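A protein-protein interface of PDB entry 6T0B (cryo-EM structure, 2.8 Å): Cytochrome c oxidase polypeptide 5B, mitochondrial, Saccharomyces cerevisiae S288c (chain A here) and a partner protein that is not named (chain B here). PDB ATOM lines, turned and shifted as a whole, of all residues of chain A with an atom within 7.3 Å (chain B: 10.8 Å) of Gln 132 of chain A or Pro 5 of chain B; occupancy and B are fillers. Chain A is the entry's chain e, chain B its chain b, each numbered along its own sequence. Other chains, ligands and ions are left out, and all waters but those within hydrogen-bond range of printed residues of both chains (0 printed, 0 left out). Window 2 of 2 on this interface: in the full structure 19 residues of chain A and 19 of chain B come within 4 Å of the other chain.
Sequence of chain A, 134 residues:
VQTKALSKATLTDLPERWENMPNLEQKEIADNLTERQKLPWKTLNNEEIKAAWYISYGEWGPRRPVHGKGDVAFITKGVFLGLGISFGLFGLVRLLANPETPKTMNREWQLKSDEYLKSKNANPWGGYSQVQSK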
ATOM      1  N   THR A 104     -13.685   0.498 -28.559  1.00  0.00           N
ATOM      2  CA  THR A 104     -13.626   1.615 -27.643  1.00  0.00           C
ATOM      3  C   THR A 104     -12.743   2.746 -28.138  1.00  0.00           C
ATOM      4  O   THR A 104     -12.746   3.819 -27.532  1.00  0.00           O
ATOM      5  CB  THR A 104     -13.130   1.129 -26.294  1.00  0.00           C
ATOM      6  OG1 THR A 104     -11.764   0.733 -26.414  1.00  0.00           O
ATOM      7  CG2 THR A 104     -13.940  -0.058 -25.859  1.00  0.00           C
ATOM      8  N   MET A 105     -11.992   2.544 -29.211  1.00  0.00           N
ATOM      9  CA  MET A 105     -11.032   3.544 -29.661  1.00  0.00           C
ATOM     10  C   MET A 105     -11.615   4.432 -30.753  1.00  0.00           C
ATOM     11  O   MET A 105     -11.028   4.622 -31.805  1.00  0.00           O
ATOM     12  CB  MET A 105      -9.760   2.867 -30.130  1.00  0.00           C
ATOM     13  CG  MET A 105      -9.048   2.150 -29.038  1.00  0.00           C
ATOM     14  SD  MET A 105      -8.160   3.312 -28.027  1.00  0.00           S
ATOM     15  CE  MET A 105      -7.163   4.101 -29.265  1.00  0.00           C
ATOM     16  N   ASN A 106     -12.778   5.006 -30.486  1.00  0.00           N
ATOM     17  CA  ASN A 106     -13.280   6.080 -31.323  1.00  0.00           C
ATOM     18  C   ASN A 106     -13.779   7.194 -30.420  1.00  0.00           C
ATOM     19  O   ASN A 106     -13.787   7.061 -29.196  1.00  0.00           O
ATOM     20  CB  ASN A 106     -14.336   5.582 -32.315  1.00  0.00           C
ATOM     21  CG  ASN A 106     -15.479   4.872 -31.663  1.00  0.00           C
ATOM     22  OD1 ASN A 106     -15.563   4.772 -30.456  1.00  0.00           O
ATOM     23  ND2 ASN A 106     -16.390   4.376 -32.478  1.00  0.00           N
ATOM     24  N   ARG A 107     -14.177   8.308 -31.029  1.00  0.00           N
ATOM     25  CA  ARG A 107     -14.509   9.488 -30.246  1.00  0.00           C
ATOM     26  C   ARG A 107     -15.804   9.311 -29.477  1.00  0.00           C
ATOM     27  O   ARG A 107     -15.918   9.785 -28.340  1.00  0.00           O
ATOM     28  CB  ARG A 107     -14.605  10.703 -31.156  1.00  0.00           C
ATOM     29  CG  ARG A 107     -14.768  11.991 -30.418  1.00  0.00           C
ATOM     30  CD  ARG A 107     -14.954  13.137 -31.349  1.00  0.00           C
ATOM     31  NE  ARG A 107     -15.195  14.355 -30.603  1.00  0.00           N
ATOM     32  CZ  ARG A 107     -14.238  15.187 -30.225  1.00  0.00           C
ATOM     33  NH1 ARG A 107     -12.982  14.929 -30.545  1.00  0.00           N
ATOM     34  NH2 ARG A 107     -14.540  16.276 -29.535  1.00  0.00           N
ATOM     35  N   GLN A 110     -15.537   7.306 -26.248  1.00  0.00           N
ATOM     36  CA  GLN A 110     -14.786   7.992 -25.217  1.00  0.00           C
ATOM     37  C   GLN A 110     -15.562   9.158 -24.633  1.00  0.00           C
ATOM     38  O   GLN A 110     -15.439   9.430 -23.435  1.00  0.00           O
ATOM     39  CB  GLN A 110     -13.446   8.409 -25.791  1.00  0.00           C
ATOM     40  CG  GLN A 110     -12.559   7.213 -26.010  1.00  0.00           C
ATOM     41  CD  GLN A 110     -11.555   7.410 -27.092  1.00  0.00           C
ATOM     42  OE1 GLN A 110     -11.564   8.407 -27.787  1.00  0.00           O
ATOM     43  NE2 GLN A 110     -10.680   6.447 -27.250  1.00  0.00           N
ATOM     44  N   ASP A 114     -16.596   9.385 -20.711  1.00  0.00           N
ATOM     45  CA  ASP A 114     -16.481  10.590 -19.910  1.00  0.00           C
ATOM     46  C   ASP A 114     -17.809  11.017 -19.336  1.00  0.00           C
ATOM     47  O   ASP A 114     -17.821  11.711 -18.318  1.00  0.00           O
ATOM     48  CB  ASP A 114     -15.936  11.738 -20.746  1.00  0.00           C
ATOM     49  CG  ASP A 114     -14.578  11.470 -21.277  1.00  0.00           C
ATOM     50  OD1 ASP A 114     -14.003  10.438 -20.911  1.00  0.00           O
ATOM     51  OD2 ASP A 114     -14.100  12.277 -22.099  1.00  0.00           O
ATOM     52  N   TYR A 128     -10.502  13.922 -16.221  1.00  0.00           N
ATOM     53  CA  TYR A 128     -11.041  12.587 -16.389  1.00  0.00           C
ATOM     54  C   TYR A 128     -11.243  12.194 -17.837  1.00  0.00           C
ATOM     55  O   TYR A 128     -11.624  11.052 -18.096  1.00  0.00           O
ATOM     56  CB  TYR A 128     -12.371  12.454 -15.649  1.00  0.00           C
ATOM     57  CG  TYR A 128     -13.406  13.499 -15.987  1.00  0.00           C
ATOM     58  CD1 TYR A 128     -14.283  13.321 -17.039  1.00  0.00           C
ATOM     59  CD2 TYR A 128     -13.529  14.642 -15.224  1.00  0.00           C
ATOM     60  CE1 TYR A 128     -15.225  14.264 -17.341  1.00  0.00           C
ATOM     61  CE2 TYR A 128     -14.475  15.591 -15.519  1.00  0.00           C
ATOM     62  CZ  TYR A 128     -15.318  15.396 -16.582  1.00  0.00           C
ATOM     63  OH  TYR A 128     -16.269  16.335 -16.887  1.00  0.00           O
ATOM     64  N   SER A 129     -11.005  13.097 -18.778  1.00  0.00           N
ATOM     65  CA  SER A 129     -11.500  12.908 -20.134  1.00  0.00           C
ATOM     66  C   SER A 129     -10.688  11.872 -20.886  1.00  0.00           C
ATOM     67  O   SER A 129      -9.457  11.890 -20.856  1.00  0.00           O
ATOM     68  CB  SER A 129     -11.486  14.222 -20.897  1.00  0.00           C
ATOM     69  OG  SER A 129     -11.767  13.984 -22.263  1.00  0.00           O
ATOM     70  N   GLN A 130     -11.384  10.979 -21.577  1.00  0.00           N
ATOM     71  CA  GLN A 130     -10.768   9.812 -22.177  1.00  0.00           C
ATOM     72  C   GLN A 130     -10.631   9.908 -23.676  1.00  0.00           C
ATOM     73  O   GLN A 130     -10.231   8.930 -24.299  1.00  0.00           O
ATOM     74  CB  GLN A 130     -11.566   8.556 -21.842  1.00  0.00           C
ATOM     75  CG  GLN A 130     -11.632   8.246 -20.375  1.00  0.00           C
ATOM     76  CD  GLN A 130     -10.409   7.540 -19.894  1.00  0.00           C
ATOM     77  OE1 GLN A 130      -9.950   6.587 -20.511  1.00  0.00           O
ATOM     78  NE2 GLN A 130      -9.869   7.994 -18.781  1.00  0.00           N
ATOM     79  N   VAL A 131     -10.954  11.040 -24.281  1.00  0.00           N
ATOM     80  CA  VAL A 131     -10.974  11.090 -25.734  1.00  0.00           C
ATOM     81  C   VAL A 131      -9.571  11.358 -26.259  1.00  0.00           C
ATOM     82  O   VAL A 131      -8.904  12.315 -25.866  1.00  0.00           O
ATOM     83  CB  VAL A 131     -12.025  12.086 -26.254  1.00  0.00           C
ATOM     84  CG1 VAL A 131     -11.835  13.491 -25.745  1.00  0.00           C
ATOM     85  CG2 VAL A 131     -12.075  12.059 -27.747  1.00  0.00           C
ATOM     86  N   GLN A 132      -9.080  10.435 -27.063  1.00  0.00           N
ATOM     87  CA  GLN A 132      -7.788  10.540 -27.699  1.00  0.00           C
ATOM     88  C   GLN A 132      -7.819  10.123 -29.149  1.00  0.00           C
ATOM     89  O   GLN A 132      -6.810  10.291 -29.833  1.00  0.00           O
ATOM     90  CB  GLN A 132      -6.756   9.683 -26.967  1.00  0.00           C
ATOM     91  CG  GLN A 132      -6.831   8.215 -27.305  1.00  0.00           C
ATOM     92  CD  GLN A 132      -6.348   7.348 -26.191  1.00  0.00           C
ATOM     93  OE1 GLN A 132      -7.138   6.815 -25.428  1.00  0.00           O
ATOM     94  NE2 GLN A 132      -5.045   7.202 -26.083  1.00  0.00           N
ATOM     95  N   SER A 133      -8.919   9.575 -29.637  1.00  0.00           N
ATOM     96  CA  SER A 133      -9.044   9.132 -31.008  1.00  0.00           C
ATOM     97  C   SER A 133      -9.965  10.068 -31.765  1.00  0.00           C
ATOM     98  O   SER A 133     -10.454  11.062 -31.232  1.00  0.00           O
ATOM     99  CB  SER A 133      -9.560   7.702 -31.064  1.00  0.00           C
ATOM    100  OG  SER A 133      -8.610   6.819 -30.519  1.00  0.00           O
ATOM    101  N   LYS A 134     -10.188   9.741 -33.027  1.00  0.00           N
ATOM    102  CA  LYS A 134     -11.058  10.536 -33.872  1.00  0.00           C
ATOM    103  C   LYS A 134     -12.382   9.822 -34.098  1.00  0.00           C
ATOM    104  O   LYS A 134     -13.208  10.261 -34.900  1.00  0.00           O
ATOM    105  CB  LYS A 134     -10.382  10.827 -35.206  1.00  0.00           C
ATOM    106  CG  LYS A 134     -10.039   9.590 -35.997  1.00  0.00           C
ATOM    107  CD  LYS A 134      -9.845   9.923 -37.464  1.00  0.00           C
ATOM    108  CE  LYS A 134      -8.703  10.907 -37.660  1.00  0.00           C
ATOM    109  NZ  LYS A 134      -7.378  10.247 -37.512  1.00  0.00           N
ATOM    110  N   VAL B   2      -8.895   7.101 -12.420  1.00  0.00           N
ATOM    111  CA  VAL B   2      -8.810   6.355 -13.668  1.00  0.00           C
ATOM    112  C   VAL B   2      -7.641   6.934 -14.456  1.00  0.00           C
ATOM    113  O   VAL B   2      -7.356   8.134 -14.340  1.00  0.00           O
ATOM    114  CB  VAL B   2     -10.153   6.405 -14.422  1.00  0.00           C
ATOM    115  CG1 VAL B   2     -10.507   7.810 -14.861  1.00  0.00           C
ATOM    116  CG2 VAL B   2     -10.170   5.474 -15.587  1.00  0.00           C
ATOM    117  N   PRO B   3      -6.880   6.129 -15.185  1.00  0.00           N
ATOM    118  CA  PRO B   3      -5.850   6.693 -16.050  1.00  0.00           C
ATOM    119  C   PRO B   3      -6.446   7.469 -17.203  1.00  0.00           C
ATOM    120  O   PRO B   3      -7.510   7.139 -17.726  1.00  0.00           O
ATOM    121  CB  PRO B   3      -5.100   5.461 -16.550  1.00  0.00           C
ATOM    122  CG  PRO B   3      -5.993   4.346 -16.284  1.00  0.00           C
ATOM    123  CD  PRO B   3      -6.688   4.687 -15.037  1.00  0.00           C
ATOM    124  N   THR B   4      -5.762   8.514 -17.575  1.00  0.00           N
ATOM    125  CA  THR B   4      -6.120   9.374 -18.671  1.00  0.00           C
ATOM    126  C   THR B   4      -5.090   9.238 -19.781  1.00  0.00           C
ATOM    127  O   THR B   4      -3.952   8.846 -19.512  1.00  0.00           O
ATOM    128  CB  THR B   4      -6.196  10.825 -18.198  1.00  0.00           C
ATOM    129  OG1 THR B   4      -4.920  11.234 -17.727  1.00  0.00           O
ATOM    130  CG2 THR B   4      -7.143  10.923 -17.077  1.00  0.00           C
ATOM    131  N   PRO B   5      -5.457   9.494 -21.037  1.00  0.00           N
ATOM    132  CA  PRO B   5      -4.483   9.357 -22.116  1.00  0.00           C
ATOM    133  C   PRO B   5      -3.418  10.425 -22.031  1.00  0.00           C
ATOM    134  O   PRO B   5      -3.697  11.568 -21.665  1.00  0.00           O
ATOM    135  CB  PRO B   5      -5.336   9.509 -23.374  1.00  0.00           C
ATOM    136  CG  PRO B   5      -6.485  10.261 -22.926  1.00  0.00           C
ATOM    137  CD  PRO B   5      -6.793   9.740 -21.590  1.00  0.00           C
ATOM    138  N   TYR B   6      -2.184  10.013 -22.315  1.00  0.00           N
ATOM    139  CA  TYR B   6      -0.980  10.837 -22.323  1.00  0.00           C
ATOM    140  C   TYR B   6      -0.648  11.427 -20.971  1.00  0.00           C
ATOM    141  O   TYR B   6       0.075  12.413 -20.908  1.00  0.00           O
ATOM    142  CB  TYR B   6      -1.052  11.970 -23.345  1.00  0.00           C
ATOM    143  CG  TYR B   6      -0.762  11.550 -24.742  1.00  0.00           C
ATOM    144  CD1 TYR B   6       0.525  11.370 -25.166  1.00  0.00           C
ATOM    145  CD2 TYR B   6      -1.783  11.346 -25.639  1.00  0.00           C
ATOM    146  CE1 TYR B   6       0.791  10.995 -26.436  1.00  0.00           C
ATOM    147  CE2 TYR B   6      -1.528  10.967 -26.906  1.00  0.00           C
ATOM    148  CZ  TYR B   6      -0.241  10.796 -27.303  1.00  0.00           C
ATOM    149  OH  TYR B   6       0.011  10.411 -28.587  1.00  0.00           O
ATOM    150  N   ALA B   7      -1.123  10.843 -19.882  1.00  0.00           N
ATOM    151  CA  ALA B   7      -0.816  11.386 -18.573  1.00  0.00           C
ATOM    152  C   ALA B   7       0.631  11.125 -18.205  1.00  0.00           C
ATOM    153  O   ALA B   7       1.288  10.242 -18.747  1.00  0.00           O
ATOM    154  CB  ALA B   7      -1.715  10.783 -17.515  1.00  0.00           C
ATOM    155  N   CYS B   8       1.122  11.921 -17.273  1.00  0.00           N
ATOM    156  CA  CYS B   8       2.508  11.853 -16.856  1.00  0.00           C
ATOM    157  C   CYS B   8       2.671  11.984 -15.358  1.00  0.00           C
ATOM    158  O   CYS B   8       3.804  12.013 -14.884  1.00  0.00           O
ATOM    159  CB  CYS B   8       3.332  12.949 -17.531  1.00  0.00           C
ATOM    160  SG  CYS B   8       3.486  12.819 -19.302  1.00  0.00           S
ATOM    161  N   TYR B   9       1.589  12.085 -14.606  1.00  0.00           N
ATOM    162  CA  TYR B   9       1.623  12.250 -13.171  1.00  0.00           C
ATOM    163  C   TYR B   9       0.776  11.153 -12.544  1.00  0.00           C
ATOM    164  O   TYR B   9       0.224  10.299 -13.237  1.00  0.00           O
ATOM    165  CB  TYR B   9       1.127  13.644 -12.779  1.00  0.00           C
ATOM    166  CG  TYR B   9       1.561  14.110 -11.419  1.00  0.00           C
ATOM    167  CD1 TYR B   9       2.878  14.026 -11.032  1.00  0.00           C
ATOM    168  CD2 TYR B   9       0.646  14.606 -10.518  1.00  0.00           C
ATOM    169  CE1 TYR B   9       3.272  14.436  -9.798  1.00  0.00           C
ATOM    170  CE2 TYR B   9       1.030  15.018  -9.282  1.00  0.00           C
ATOM    171  CZ  TYR B   9       2.343  14.932  -8.928  1.00  0.00           C
ATOM    172  OH  TYR B   9       2.735  15.349  -7.685  1.00  0.00           O
ATOM    173  N   PHE B  10       0.708  11.161 -11.222  1.00  0.00           N
ATOM    174  CA  PHE B  10      -0.118  10.236 -10.478  1.00  0.00           C
ATOM    175  C   PHE B  10      -1.588  10.433 -10.802  1.00  0.00           C
ATOM    176  O   PHE B  10      -2.016  11.486 -11.272  1.00  0.00           O
ATOM    177  CB  PHE B  10       0.072  10.441  -8.985  1.00  0.00           C
ATOM    178  CG  PHE B  10       1.350   9.910  -8.468  1.00  0.00           C
ATOM    179  CD1 PHE B  10       1.533   8.558  -8.337  1.00  0.00           C
ATOM    180  CD2 PHE B  10       2.363  10.761  -8.096  1.00  0.00           C
ATOM    181  CE1 PHE B  10       2.706   8.063  -7.856  1.00  0.00           C
ATOM    182  CE2 PHE B  10       3.538  10.272  -7.612  1.00  0.00           C
ATOM    183  CZ  PHE B  10       3.711   8.923  -7.493  1.00  0.00           C
ATOM    184  N   GLN B  11      -2.369   9.395 -10.540  1.00  0.00           N
ATOM    185  CA  GLN B  11      -3.804   9.576 -10.487  1.00  0.00           C
ATOM    186  C   GLN B  11      -4.167  10.400  -9.260  1.00  0.00           C
ATOM    187  O   GLN B  11      -3.393  10.518  -8.308  1.00  0.00           O
ATOM    188  CB  GLN B  11      -4.512   8.229 -10.459  1.00  0.00           C
ATOM    189  CG  GLN B  11      -4.316   7.441 -11.703  1.00  0.00           C
ATOM    190  CD  GLN B  11      -4.910   6.079 -11.609  1.00  0.00           C
ATOM    191  OE1 GLN B  11      -5.973   5.896 -11.037  1.00  0.00           O
ATOM    192  NE2 GLN B  11      -4.224   5.100 -12.166  1.00  0.00           N
ATOM    193  N   LEU B 143     -15.441   1.112 -19.989  1.00  0.00           N
ATOM    194  CA  LEU B 143     -14.000   1.268 -20.077  1.00  0.00           C
ATOM    195  C   LEU B 143     -13.370  -0.098 -20.259  1.00  0.00           C
ATOM    196  O   LEU B 143     -13.522  -0.971 -19.403  1.00  0.00           O
ATOM    197  CB  LEU B 143     -13.457   1.939 -18.825  1.00  0.00           C
ATOM    198  CG  LEU B 143     -13.725   3.428 -18.655  1.00  0.00           C
ATOM    199  CD1 LEU B 143     -15.043   3.704 -17.957  1.00  0.00           C
ATOM    200  CD2 LEU B 143     -12.621   4.030 -17.879  1.00  0.00           C
ATOM    201  N   ARG B 144     -12.653  -0.274 -21.358  1.00  0.00           N
ATOM    202  CA  ARG B 144     -12.117  -1.578 -21.706  1.00  0.00           C
ATOM    203  C   ARG B 144     -10.970  -1.947 -20.788  1.00  0.00           C
ATOM    204  O   ARG B 144     -10.161  -1.097 -20.417  1.00  0.00           O
ATOM    205  CB  ARG B 144     -11.644  -1.574 -23.146  1.00  0.00           C
ATOM    206  CG  ARG B 144     -11.522  -2.926 -23.758  1.00  0.00           C
ATOM    207  CD  ARG B 144     -10.889  -2.807 -25.115  1.00  0.00           C
ATOM    208  NE  ARG B 144      -9.485  -2.458 -24.987  1.00  0.00           N
ATOM    209  CZ  ARG B 144      -8.506  -3.347 -25.022  1.00  0.00           C
ATOM    210  NH1 ARG B 144      -7.254  -2.960 -24.895  1.00  0.00           N
ATOM    211  NH2 ARG B 144      -8.786  -4.624 -25.198  1.00  0.00           N
ATOM    212  N   LEU B 146     -10.975  -2.455 -17.752  1.00  0.00           N
ATOM    213  CA  LEU B 146     -11.075  -1.858 -16.438  1.00  0.00           C
ATOM    214  C   LEU B 146     -12.401  -2.153 -15.776  1.00  0.00           C
ATOM    215  O   LEU B 146     -12.446  -2.327 -14.559  1.00  0.00           O
ATOM    216  CB  LEU B 146     -10.881  -0.366 -16.526  1.00  0.00           C
ATOM    217  CG  LEU B 146      -9.442   0.090 -16.627  1.00  0.00           C
ATOM    218  CD1 LEU B 146      -9.413   1.562 -16.935  1.00  0.00           C
ATOM    219  CD2 LEU B 146      -8.708  -0.207 -15.341  1.00  0.00           C
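The backbone carbonyl oxygen of Pro 3 of chain B sits at hydrogen-bond distance from the side-chain amide nitrogen of Gln 130 of chain A, 2.7 Å away.
Arg 144 of chain B touches Thr 104 of chain A. Ser 129 of chain A touches Pro 5 of chain B (O to CD, 3.5 Å). Gln 130 of chain A touches Val 2 of chain B. NE2 of Gln 130 of chain A touches CA of Thr 4 of chain B (3.996 Å). Gln 132 of chain A touches Pro 5 of chain B (NE2 to CB, 3.6 Å).
Of the 13 printed residues of chain B, 5 touch a printed residue of chain A. Along chain B the printed residues that touch a printed residue of chain A span positions 2 to 144. Printed residues of chain A that touch a printed residue of chain B: Thr 104, Ser 129, Gln 130 and Gln 132. Among the printed residues, 6 pairs touch across the chains. Among the printed residues, no Asp or Glu carboxylate lies within 4 Å of a Lys or Arg side-chain nitrogen of the other chain.
The side-chain carboxylate (OD1) of Asp 114 of chain A lies within hydrogen-bond range of the backbone NH (N) of Gln 130 of chain A (2.8 Å). The side-chain amide nitrogen (NE2) of Gln 110 of chain A sits at hydrogen-bond distance from the backbone carbonyl oxygen (O) of Thr 104 of chain A, at 3.4 Å. The side-chain amide oxygen of Gln 110 of chain A lies within hydrogen-bond range of the backbone NH of Gln 132 of chain A. The side-chain amide oxygen (OE1) of Gln 11 of chain B sits at hydrogen-bond distance from the backbone NH (N) of Val 2 of chain B, 3.5 Å away. The side-chain hydroxyl (OG) of Ser 129 of chain A sits at hydrogen-bond distance from the side-chain carboxylate (OD2) of Asp 114 of chain A (2.9 Å).
Of the printed residues of chain B, Thr 104 of chain A touches Arg 144. Ser 129 of chain A touches one residue of chain B. No residue of chain B comes within 4 Å of Val 131 of chain A. No residue of chain B comes within 4 Å of Ser 133 of chain A. Printed residues of chain A within 4 Å of Pro 5 of chain B: Ser 129 (3.5 Å) and Gln 132 (3.6 Å). Cys 8 of chain B touches none of the printed residues of chain A. Gln 11 of chain B touches none of the printed residues of chain A. Of the printed residues of chain A, Arg 144 of chain B touches Thr 104. The nearest printed residue of chain A that does not touch Pro 5 of chain B is Gln 130 of chain A (4.02 Å). The nearest printed residue of chain B that does not touch Gln 130 of chain A is Pro 5 of chain B (4.02 Å).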
